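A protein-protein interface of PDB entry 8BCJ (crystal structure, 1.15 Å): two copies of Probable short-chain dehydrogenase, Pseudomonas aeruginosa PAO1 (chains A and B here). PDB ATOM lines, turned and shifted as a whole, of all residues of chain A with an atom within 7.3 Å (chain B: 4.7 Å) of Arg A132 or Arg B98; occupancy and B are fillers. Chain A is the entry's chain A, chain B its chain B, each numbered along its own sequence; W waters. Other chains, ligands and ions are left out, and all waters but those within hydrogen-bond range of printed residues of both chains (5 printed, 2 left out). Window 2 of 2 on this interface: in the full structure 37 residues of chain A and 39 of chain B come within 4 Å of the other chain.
Water W5 bridges OE2 of Glu B100 (2.6 Å) and OE1 of Glu A180 (3.0 Å). Water W3 lies within hydrogen-bond range of OE2 of Glu A176, N of Glu B100 and N of Leu B99. Water W1 lies within hydrogen-bond range of the backbone carbonyl oxygen (O) of Thr B97 (2.9 Å) and the side-chain carboxylate (OE1) of Glu A176 (2.9 Å). Water W4 bridges OE1 of Glu B100 (2.9 Å) and NE2 of His A133 (3.2 Å). Water W2 lies within hydrogen-bond range of the side-chain amino group (NZ) of Lys A127 (2.9 Å), the guanidinium group (NH2) of Arg A123 (3.0 Å), the backbone carbonyl oxygen (O) of Glu B100 (3.0 Å) and the side-chain amide oxygen (OD1) of Asn B101 (3.3 Å).
O of Leu B99 touches CD of Arg A123 (3.6 Å). O of Glu B100 touches CE of Lys A127 (3.4 Å). Leu B99 touches Leu A173. OE2 of Glu A176 touches CA of Arg B98, at 3.5 Å.
N of Arg A132 lies within hydrogen-bond range of OG of Ser A130 (2.9 Å). OE2 of Glu A180 lies within salt-bridge range of NE of Arg A132 (3.2 Å).
The guanidinium group of Arg A123 sits at hydrogen-bond distance from the backbone carbonyl oxygen of Glu B100 (2.9 Å). The side-chain carboxylate of Glu A176 is in hydrogen-bond range of the backbone NH of Asn B154 (2.7 Å). OE1 of Glu B100 lies within hydrogen-bond range of NE2 of His A133, at 2.7 Å. NE of Arg A123 sits close to O of Ile B102 (3.4 Å). NH1 of Arg B98 sits close to NH2 of Arg A132, 3.0 Å away. The side-chain carboxylate (OE2) of Glu A176 lies within hydrogen-bond range of the backbone NH (N) of Leu B99, at 2.7 Å.
Of the printed residues of chain B, Arg A123 touches Leu B99, Glu B100 and Ile B102. Of the printed residues of chain B, Arg A132 touches Arg B98 (3.0 Å). Of the printed residues of chain B, Leu A173 touches Leu B99. Of the printed residues of chain B, Glu A176 touches Arg B98, Leu B99 and Asn B154. Of the printed residues of chain A, Arg B98 touches Arg A132 (3.0 Å) and Glu A176 (3.5 Å). Printed residues of chain A within 4 Å of Asn B154: Glu A176. The nearest printed residue of chain B that does not touch Glu A176 is Thr B97 (4.02 Å).
Of the 7 printed residues of chain B, 5 touch a printed residue of chain A. Hydrophobic or aromatic side chains of chain B that line the printed part of chain A: Leu B99. Of the 16 printed residues of chain A, 6 touch a printed residue of chain B. Printed residues of chain A that touch a printed residue of chain B: Arg A123, Lys A127, Arg A132, His A133, Leu A173 and Glu A176. Hydrophobic or aromatic side chains of chain A within 4 Å of the printed part of chain B: His A133 and Leu A173. Among the printed residues, no Asp or Glu carboxylate lies within 4 Å of a Lys or Arg side-chain nitrogen of the other chain.
No position is printed for both chains. Of the 10 pairs that touch across the chains among the printed residues, none has its exchanged pair printed and touching as well.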
ATOM      1  N   ARG A 123       9.270 -26.820   1.901  1.00  0.00           N
ATOM      2  CA  ARG A 123       9.403 -28.009   2.740  1.00  0.00           C
ATOM      3  C   ARG A 123      10.253 -27.728   3.976  1.00  0.00           C
ATOM      4  O   ARG A 123       9.858 -28.049   5.107  1.00  0.00           O
ATOM      5  CB  ARG A 123       9.980 -29.145   1.901  1.00  0.00           C
ATOM      6  CG  ARG A 123      10.507 -30.371   2.647  1.00  0.00           C
ATOM      7  CD  ARG A 123      10.611 -31.531   1.653  1.00  0.00           C
ATOM      8  NE  ARG A 123      11.282 -32.738   2.112  1.00  0.00           N
ATOM      9  CZ  ARG A 123      12.399 -33.236   1.595  1.00  0.00           C
ATOM     10  NH1 ARG A 123      13.118 -32.564   0.718  1.00  0.00           N
ATOM     11  NH2 ARG A 123      12.792 -34.452   1.959  1.00  0.00           N
ATOM     12  N   VAL A 126       8.376 -25.385   6.298  1.00  0.00           N
ATOM     13  CA  VAL A 126       7.360 -26.088   7.087  1.00  0.00           C
ATOM     14  C   VAL A 126       8.006 -26.791   8.272  1.00  0.00           C
ATOM     15  O   VAL A 126       7.468 -26.787   9.389  1.00  0.00           O
ATOM     16  CB  VAL A 126       6.558 -27.058   6.197  1.00  0.00           C
ATOM     17  CG1 VAL A 126       5.696 -27.995   7.051  1.00  0.00           C
ATOM     18  CG2 VAL A 126       5.666 -26.280   5.254  1.00  0.00           C
ATOM     19  N   LYS A 127       9.161 -27.403   8.052  1.00  0.00           N
ATOM     20  CA  LYS A 127       9.848 -28.109   9.129  1.00  0.00           C
ATOM     21  C   LYS A 127      10.292 -27.189  10.259  1.00  0.00           C
ATOM     22  O   LYS A 127      10.566 -27.674  11.360  1.00  0.00           O
ATOM     23  CB  LYS A 127      11.038 -28.890   8.557  1.00  0.00           C
ATOM     24  CG  LYS A 127      10.624 -30.076   7.691  1.00  0.00           C
ATOM     25  CD  LYS A 127      11.821 -30.824   7.111  1.00  0.00           C
ATOM     26  CE  LYS A 127      11.382 -32.002   6.239  1.00  0.00           C
ATOM     27  NZ  LYS A 127      12.548 -32.809   5.763  1.00  0.00           N
ATOM     28  N   LEU A 129       8.590 -23.800  10.739  1.00  0.00           N
ATOM     29  CA  LEU A 129       7.454 -22.998  11.171  1.00  0.00           C
ATOM     30  C   LEU A 129       6.374 -23.841  11.829  1.00  0.00           C
ATOM     31  O   LEU A 129       5.674 -23.357  12.726  1.00  0.00           O
ATOM     32  CB  LEU A 129       6.811 -22.283   9.981  1.00  0.00           C
ATOM     33  CG  LEU A 129       7.412 -20.954   9.529  1.00  0.00           C
ATOM     34  CD1 LEU A 129       8.894 -21.085   9.186  1.00  0.00           C
ATOM     35  CD2 LEU A 129       6.618 -20.452   8.335  1.00  0.00           C
ATOM     36  N   SER A 130       6.208 -25.082  11.391  1.00  0.00           N
ATOM     37  CA  SER A 130       5.046 -25.855  11.801  1.00  0.00           C
ATOM     38  C   SER A 130       5.010 -26.051  13.304  1.00  0.00           C
ATOM     39  O   SER A 130       6.025 -26.359  13.936  1.00  0.00           O
ATOM     40  CB  SER A 130       5.057 -27.220  11.106  1.00  0.00           C
ATOM     41  OG  SER A 130       3.989 -28.026  11.586  1.00  0.00           O
ATOM     42  N   THR A 131       3.803 -25.922  13.862  1.00  0.00           N
ATOM     43  CA  THR A 131       3.578 -26.338  15.246  1.00  0.00           C
ATOM     44  C   THR A 131       3.786 -27.840  15.460  1.00  0.00           C
ATOM     45  O   THR A 131       3.859 -28.263  16.614  1.00  0.00           O
ATOM     46  CB  THR A 131       2.207 -25.852  15.737  1.00  0.00           C
ATOM     47  OG1 THR A 131       1.183 -26.381  14.907  1.00  0.00           O
ATOM     48  CG2 THR A 131       2.137 -24.326  15.703  1.00  0.00           C
ATOM     49  N   ARG A 132       3.863 -28.649  14.396  1.00  0.00           N
ATOM     50  CA  ARG A 132       4.246 -30.048  14.564  1.00  0.00           C
ATOM     51  C   ARG A 132       5.705 -30.175  15.011  1.00  0.00           C
ATOM     52  O   ARG A 132       6.065 -31.127  15.720  1.00  0.00           O
ATOM     53  CB  ARG A 132       4.094 -30.809  13.237  1.00  0.00           C
ATOM     54  CG  ARG A 132       2.669 -31.103  12.812  1.00  0.00           C
ATOM     55  CD  ARG A 132       2.612 -31.873  11.487  1.00  0.00           C
ATOM     56  NE  ARG A 132       1.236 -32.014  11.027  1.00  0.00           N
ATOM     57  CZ  ARG A 132       0.361 -32.859  11.557  1.00  0.00           C
ATOM     58  NH1 ARG A 132       0.697 -33.675  12.543  1.00  0.00           N
ATOM     59  NH2 ARG A 132      -0.880 -32.889  11.082  1.00  0.00           N
ATOM     60  N   HIS A 133       6.560 -29.226  14.611  1.00  0.00           N
ATOM     61  CA  HIS A 133       8.009 -29.400  14.633  1.00  0.00           C
ATOM     62  C   HIS A 133       8.748 -28.339  15.442  1.00  0.00           C
ATOM     63  O   HIS A 133       9.891 -27.989  15.119  1.00  0.00           O
ATOM     64  CB  HIS A 133       8.539 -29.415  13.198  1.00  0.00           C
ATOM     65  CG  HIS A 133       7.857 -30.406  12.307  1.00  0.00           C
ATOM     66  ND1 HIS A 133       7.724 -31.739  12.643  1.00  0.00           N
ATOM     67  CD2 HIS A 133       7.289 -30.266  11.085  1.00  0.00           C
ATOM     68  CE1 HIS A 133       7.093 -32.371  11.670  1.00  0.00           C
ATOM     69  NE2 HIS A 133       6.821 -31.502  10.711  1.00  0.00           N
ATOM     70  N   GLY A 134       8.127 -27.814  16.486  1.00  0.00           N
ATOM     71  CA  GLY A 134       8.791 -26.865  17.351  1.00  0.00           C
ATOM     72  C   GLY A 134       8.608 -25.419  16.959  1.00  0.00           C
ATOM     73  O   GLY A 134       9.138 -24.534  17.638  1.00  0.00           O
ATOM     74  N   GLY A 135       7.879 -25.151  15.890  1.00  0.00           N
ATOM     75  CA  GLY A 135       7.704 -23.790  15.438  1.00  0.00           C
ATOM     76  C   GLY A 135       6.526 -23.110  16.078  1.00  0.00           C
ATOM     77  O   GLY A 135       5.747 -23.717  16.811  1.00  0.00           O
ATOM     78  N   LEU A 173      -0.777 -26.223  -0.659  1.00  0.00           N
ATOM     79  CA  LEU A 173      -0.017 -26.113   0.581  1.00  0.00           C
ATOM     80  C   LEU A 173      -0.788 -25.305   1.614  1.00  0.00           C
ATOM     81  O   LEU A 173      -0.809 -25.661   2.792  1.00  0.00           O
ATOM     82  CB  LEU A 173       1.375 -25.530   0.343  1.00  0.00           C
ATOM     83  CG  LEU A 173       2.296 -25.573   1.564  1.00  0.00           C
ATOM     84  CD1 LEU A 173       2.526 -26.999   2.065  1.00  0.00           C
ATOM     85  CD2 LEU A 173       3.622 -24.921   1.233  1.00  0.00           C
ATOM     86  N   GLU A 176      -3.086 -27.611   3.167  1.00  0.00           N
ATOM     87  CA  GLU A 176      -2.408 -28.676   3.897  1.00  0.00           C
ATOM     88  C   GLU A 176      -1.867 -28.234   5.248  1.00  0.00           C
ATOM     89  O   GLU A 176      -1.922 -29.011   6.206  1.00  0.00           O
ATOM     90  CB  GLU A 176      -1.284 -29.245   3.031  1.00  0.00           C
ATOM     91  CG  GLU A 176      -0.518 -30.398   3.637  1.00  0.00           C
ATOM     92  CD  GLU A 176       0.436 -31.022   2.638  1.00  0.00           C
ATOM     93  OE1 GLU A 176      -0.010 -31.740   1.720  1.00  0.00           O
ATOM     94  OE2 GLU A 176       1.638 -30.761   2.753  1.00  0.00           O
ATOM     95  N   VAL A 177      -1.308 -27.030   5.359  1.00  0.00           N
ATOM     96  CA  VAL A 177      -0.606 -26.632   6.579  1.00  0.00           C
ATOM     97  C   VAL A 177      -1.342 -25.564   7.381  1.00  0.00           C
ATOM     98  O   VAL A 177      -0.810 -25.084   8.395  1.00  0.00           O
ATOM     99  CB  VAL A 177       0.855 -26.235   6.331  1.00  0.00           C
ATOM    100  CG1 VAL A 177       1.645 -27.422   5.818  1.00  0.00           C
ATOM    101  CG2 VAL A 177       0.981 -25.044   5.399  1.00  0.00           C
ATOM    102  N   ALA A 179      -3.626 -26.002   9.497  1.00  0.00           N
ATOM    103  CA  ALA A 179      -3.841 -26.469  10.862  1.00  0.00           C
ATOM    104  C   ALA A 179      -2.561 -26.496  11.676  1.00  0.00           C
ATOM    105  O   ALA A 179      -2.626 -26.779  12.879  1.00  0.00           O
ATOM    106  CB  ALA A 179      -4.503 -27.850  10.847  1.00  0.00           C
ATOM    107  N   GLU A 180      -1.416 -26.203  11.055  1.00  0.00           N
ATOM    108  CA  GLU A 180      -0.109 -26.173  11.701  1.00  0.00           C
ATOM    109  C   GLU A 180       0.406 -24.761  11.896  1.00  0.00           C
ATOM    110  O   GLU A 180       1.594 -24.578  12.178  1.00  0.00           O
ATOM    111  CB  GLU A 180       0.902 -26.965  10.873  1.00  0.00           C
ATOM    112  CG  GLU A 180       0.708 -28.451  10.947  1.00  0.00           C
ATOM    113  CD  GLU A 180       1.349 -29.157   9.779  1.00  0.00           C
ATOM    114  OE1 GLU A 180       2.590 -29.131   9.671  1.00  0.00           O
ATOM    115  OE2 GLU A 180       0.600 -29.721   8.960  1.00  0.00           O
ATOM    116  N   GLY A 181      -0.462 -23.769  11.750  1.00  0.00           N
ATOM    117  CA  GLY A 181      -0.111 -22.405  12.021  1.00  0.00           C
ATOM    118  C   GLY A 181       0.516 -21.656  10.884  1.00  0.00           C
ATOM    119  O   GLY A 181       1.028 -20.563  11.116  1.00  0.00           O
ATOM    120  N   THR B  97       0.961 -38.187   0.446  1.00  0.00           N
ATOM    121  CA  THR B  97       1.960 -37.656   1.351  1.00  0.00           C
ATOM    122  C   THR B  97       1.664 -36.186   1.593  1.00  0.00           C
ATOM    123  O   THR B  97       0.881 -35.568   0.884  1.00  0.00           O
ATOM    124  CB  THR B  97       3.343 -37.764   0.701  1.00  0.00           C
ATOM    125  OG1 THR B  97       4.357 -37.375   1.629  1.00  0.00           O
ATOM    126  CG2 THR B  97       3.424 -36.855  -0.519  1.00  0.00           C
ATOM    127  N   ARG B  98       2.311 -35.633   2.614  1.00  0.00           N
ATOM    128  CA  ARG B  98       2.371 -34.189   2.811  1.00  0.00           C
ATOM    129  C   ARG B  98       3.622 -33.633   2.139  1.00  0.00           C
ATOM    130  O   ARG B  98       4.588 -34.360   1.901  1.00  0.00           O
ATOM    131  CB  ARG B  98       2.332 -33.856   4.301  1.00  0.00           C
ATOM    132  CG  ARG B  98       1.014 -34.306   4.915  1.00  0.00           C
ATOM    133  CD  ARG B  98       0.803 -33.906   6.359  1.00  0.00           C
ATOM    134  NE  ARG B  98       1.598 -34.712   7.273  1.00  0.00           N
ATOM    135  CZ  ARG B  98       1.208 -35.101   8.482  1.00  0.00           C
ATOM    136  NH1 ARG B  98      -0.015 -34.864   8.932  1.00  0.00           N
ATOM    137  NH2 ARG B  98       2.069 -35.745   9.256  1.00  0.00           N
ATOM    138  N   LEU B  99       3.572 -32.325   1.808  1.00  0.00           N
ATOM    139  CA  LEU B  99       4.646 -31.680   1.047  1.00  0.00           C
ATOM    140  C   LEU B  99       5.957 -31.743   1.793  1.00  0.00           C
ATOM    141  O   LEU B  99       7.028 -31.828   1.169  1.00  0.00           O
ATOM    142  CB  LEU B  99       4.274 -30.226   0.700  1.00  0.00           C
ATOM    143  CG  LEU B  99       5.282 -29.386  -0.112  1.00  0.00           C
ATOM    144  CD1 LEU B  99       4.615 -28.425  -1.079  1.00  0.00           C
ATOM    145  CD2 LEU B  99       6.191 -28.597   0.836  1.00  0.00           C
ATOM    146  N   GLU B 100       5.910 -31.703   3.121  1.00  0.00           N
ATOM    147  CA  GLU B 100       7.153 -31.776   3.874  1.00  0.00           C
ATOM    148  C   GLU B 100       7.902 -33.083   3.645  1.00  0.00           C
ATOM    149  O   GLU B 100       9.092 -33.151   3.984  1.00  0.00           O
ATOM    150  CB  GLU B 100       6.894 -31.536   5.356  1.00  0.00           C
ATOM    151  CG  GLU B 100       6.094 -32.598   6.047  1.00  0.00           C
ATOM    152  CD  GLU B 100       6.105 -32.414   7.553  1.00  0.00           C
ATOM    153  OE1 GLU B 100       7.207 -32.268   8.121  1.00  0.00           O
ATOM    154  OE2 GLU B 100       5.016 -32.402   8.155  1.00  0.00           O
ATOM    155  N   ASN B 101       7.266 -34.093   3.036  1.00  0.00           N
ATOM    156  CA  ASN B 101       7.903 -35.372   2.756  1.00  0.00           C
ATOM    157  C   ASN B 101       8.071 -35.655   1.259  1.00  0.00           C
ATOM    158  O   ASN B 101       8.336 -36.795   0.874  1.00  0.00           O
ATOM    159  CB  ASN B 101       7.191 -36.515   3.474  1.00  0.00           C
ATOM    160  CG  ASN B 101       7.263 -36.365   4.988  1.00  0.00           C
ATOM    161  OD1 ASN B 101       8.280 -35.913   5.524  1.00  0.00           O
ATOM    162  ND2 ASN B 101       6.182 -36.713   5.678  1.00  0.00           N
ATOM    163  N   ILE B 102       7.940 -34.638   0.412  1.00  0.00           N
ATOM    164  CA  ILE B 102       8.174 -34.727  -1.032  1.00  0.00           C
ATOM    165  C   ILE B 102       9.597 -34.243  -1.289  1.00  0.00           C
ATOM    166  O   ILE B 102       9.934 -33.102  -0.948  1.00  0.00           O
ATOM    167  CB  ILE B 102       7.172 -33.854  -1.802  1.00  0.00           C
ATOM    168  CG1 ILE B 102       5.762 -34.396  -1.609  1.00  0.00           C
ATOM    169  CG2 ILE B 102       7.566 -33.751  -3.267  1.00  0.00           C
ATOM    170  CD1 ILE B 102       4.682 -33.534  -2.253  1.00  0.00           C
ATOM    171  N   ASN B 154      -2.505 -32.840   1.457  1.00  0.00           N
ATOM    172  CA  ASN B 154      -2.349 -34.081   2.208  1.00  0.00           C
ATOM    173  C   ASN B 154      -2.292 -35.301   1.302  1.00  0.00           C
ATOM    174  O   ASN B 154      -2.306 -36.441   1.806  1.00  0.00           O
ATOM    175  CB  ASN B 154      -3.433 -34.249   3.277  1.00  0.00           C
ATOM    176  CG  ASN B 154      -3.463 -33.070   4.239  1.00  0.00           C
ATOM    177  OD1 ASN B 154      -2.506 -32.824   4.935  1.00  0.00           O
ATOM    178  ND2 ASN B 154      -4.572 -32.337   4.259  1.00  0.00           N
HETATM  179  O   HOH W   1       1.012 -33.125  -0.650  1.00  0.00           O
HETATM  180  O   HOH W   2      11.292 -35.136   4.456  1.00  0.00           O
HETATM  181  O   HOH W   3       3.709 -30.368   4.540  1.00  0.00           O
HETATM  182  O   HOH W   4       9.568 -32.795   9.736  1.00  0.00           O
HETATM  183  O   HOH W   5       3.177 -30.836   7.300  1.00  0.00           O
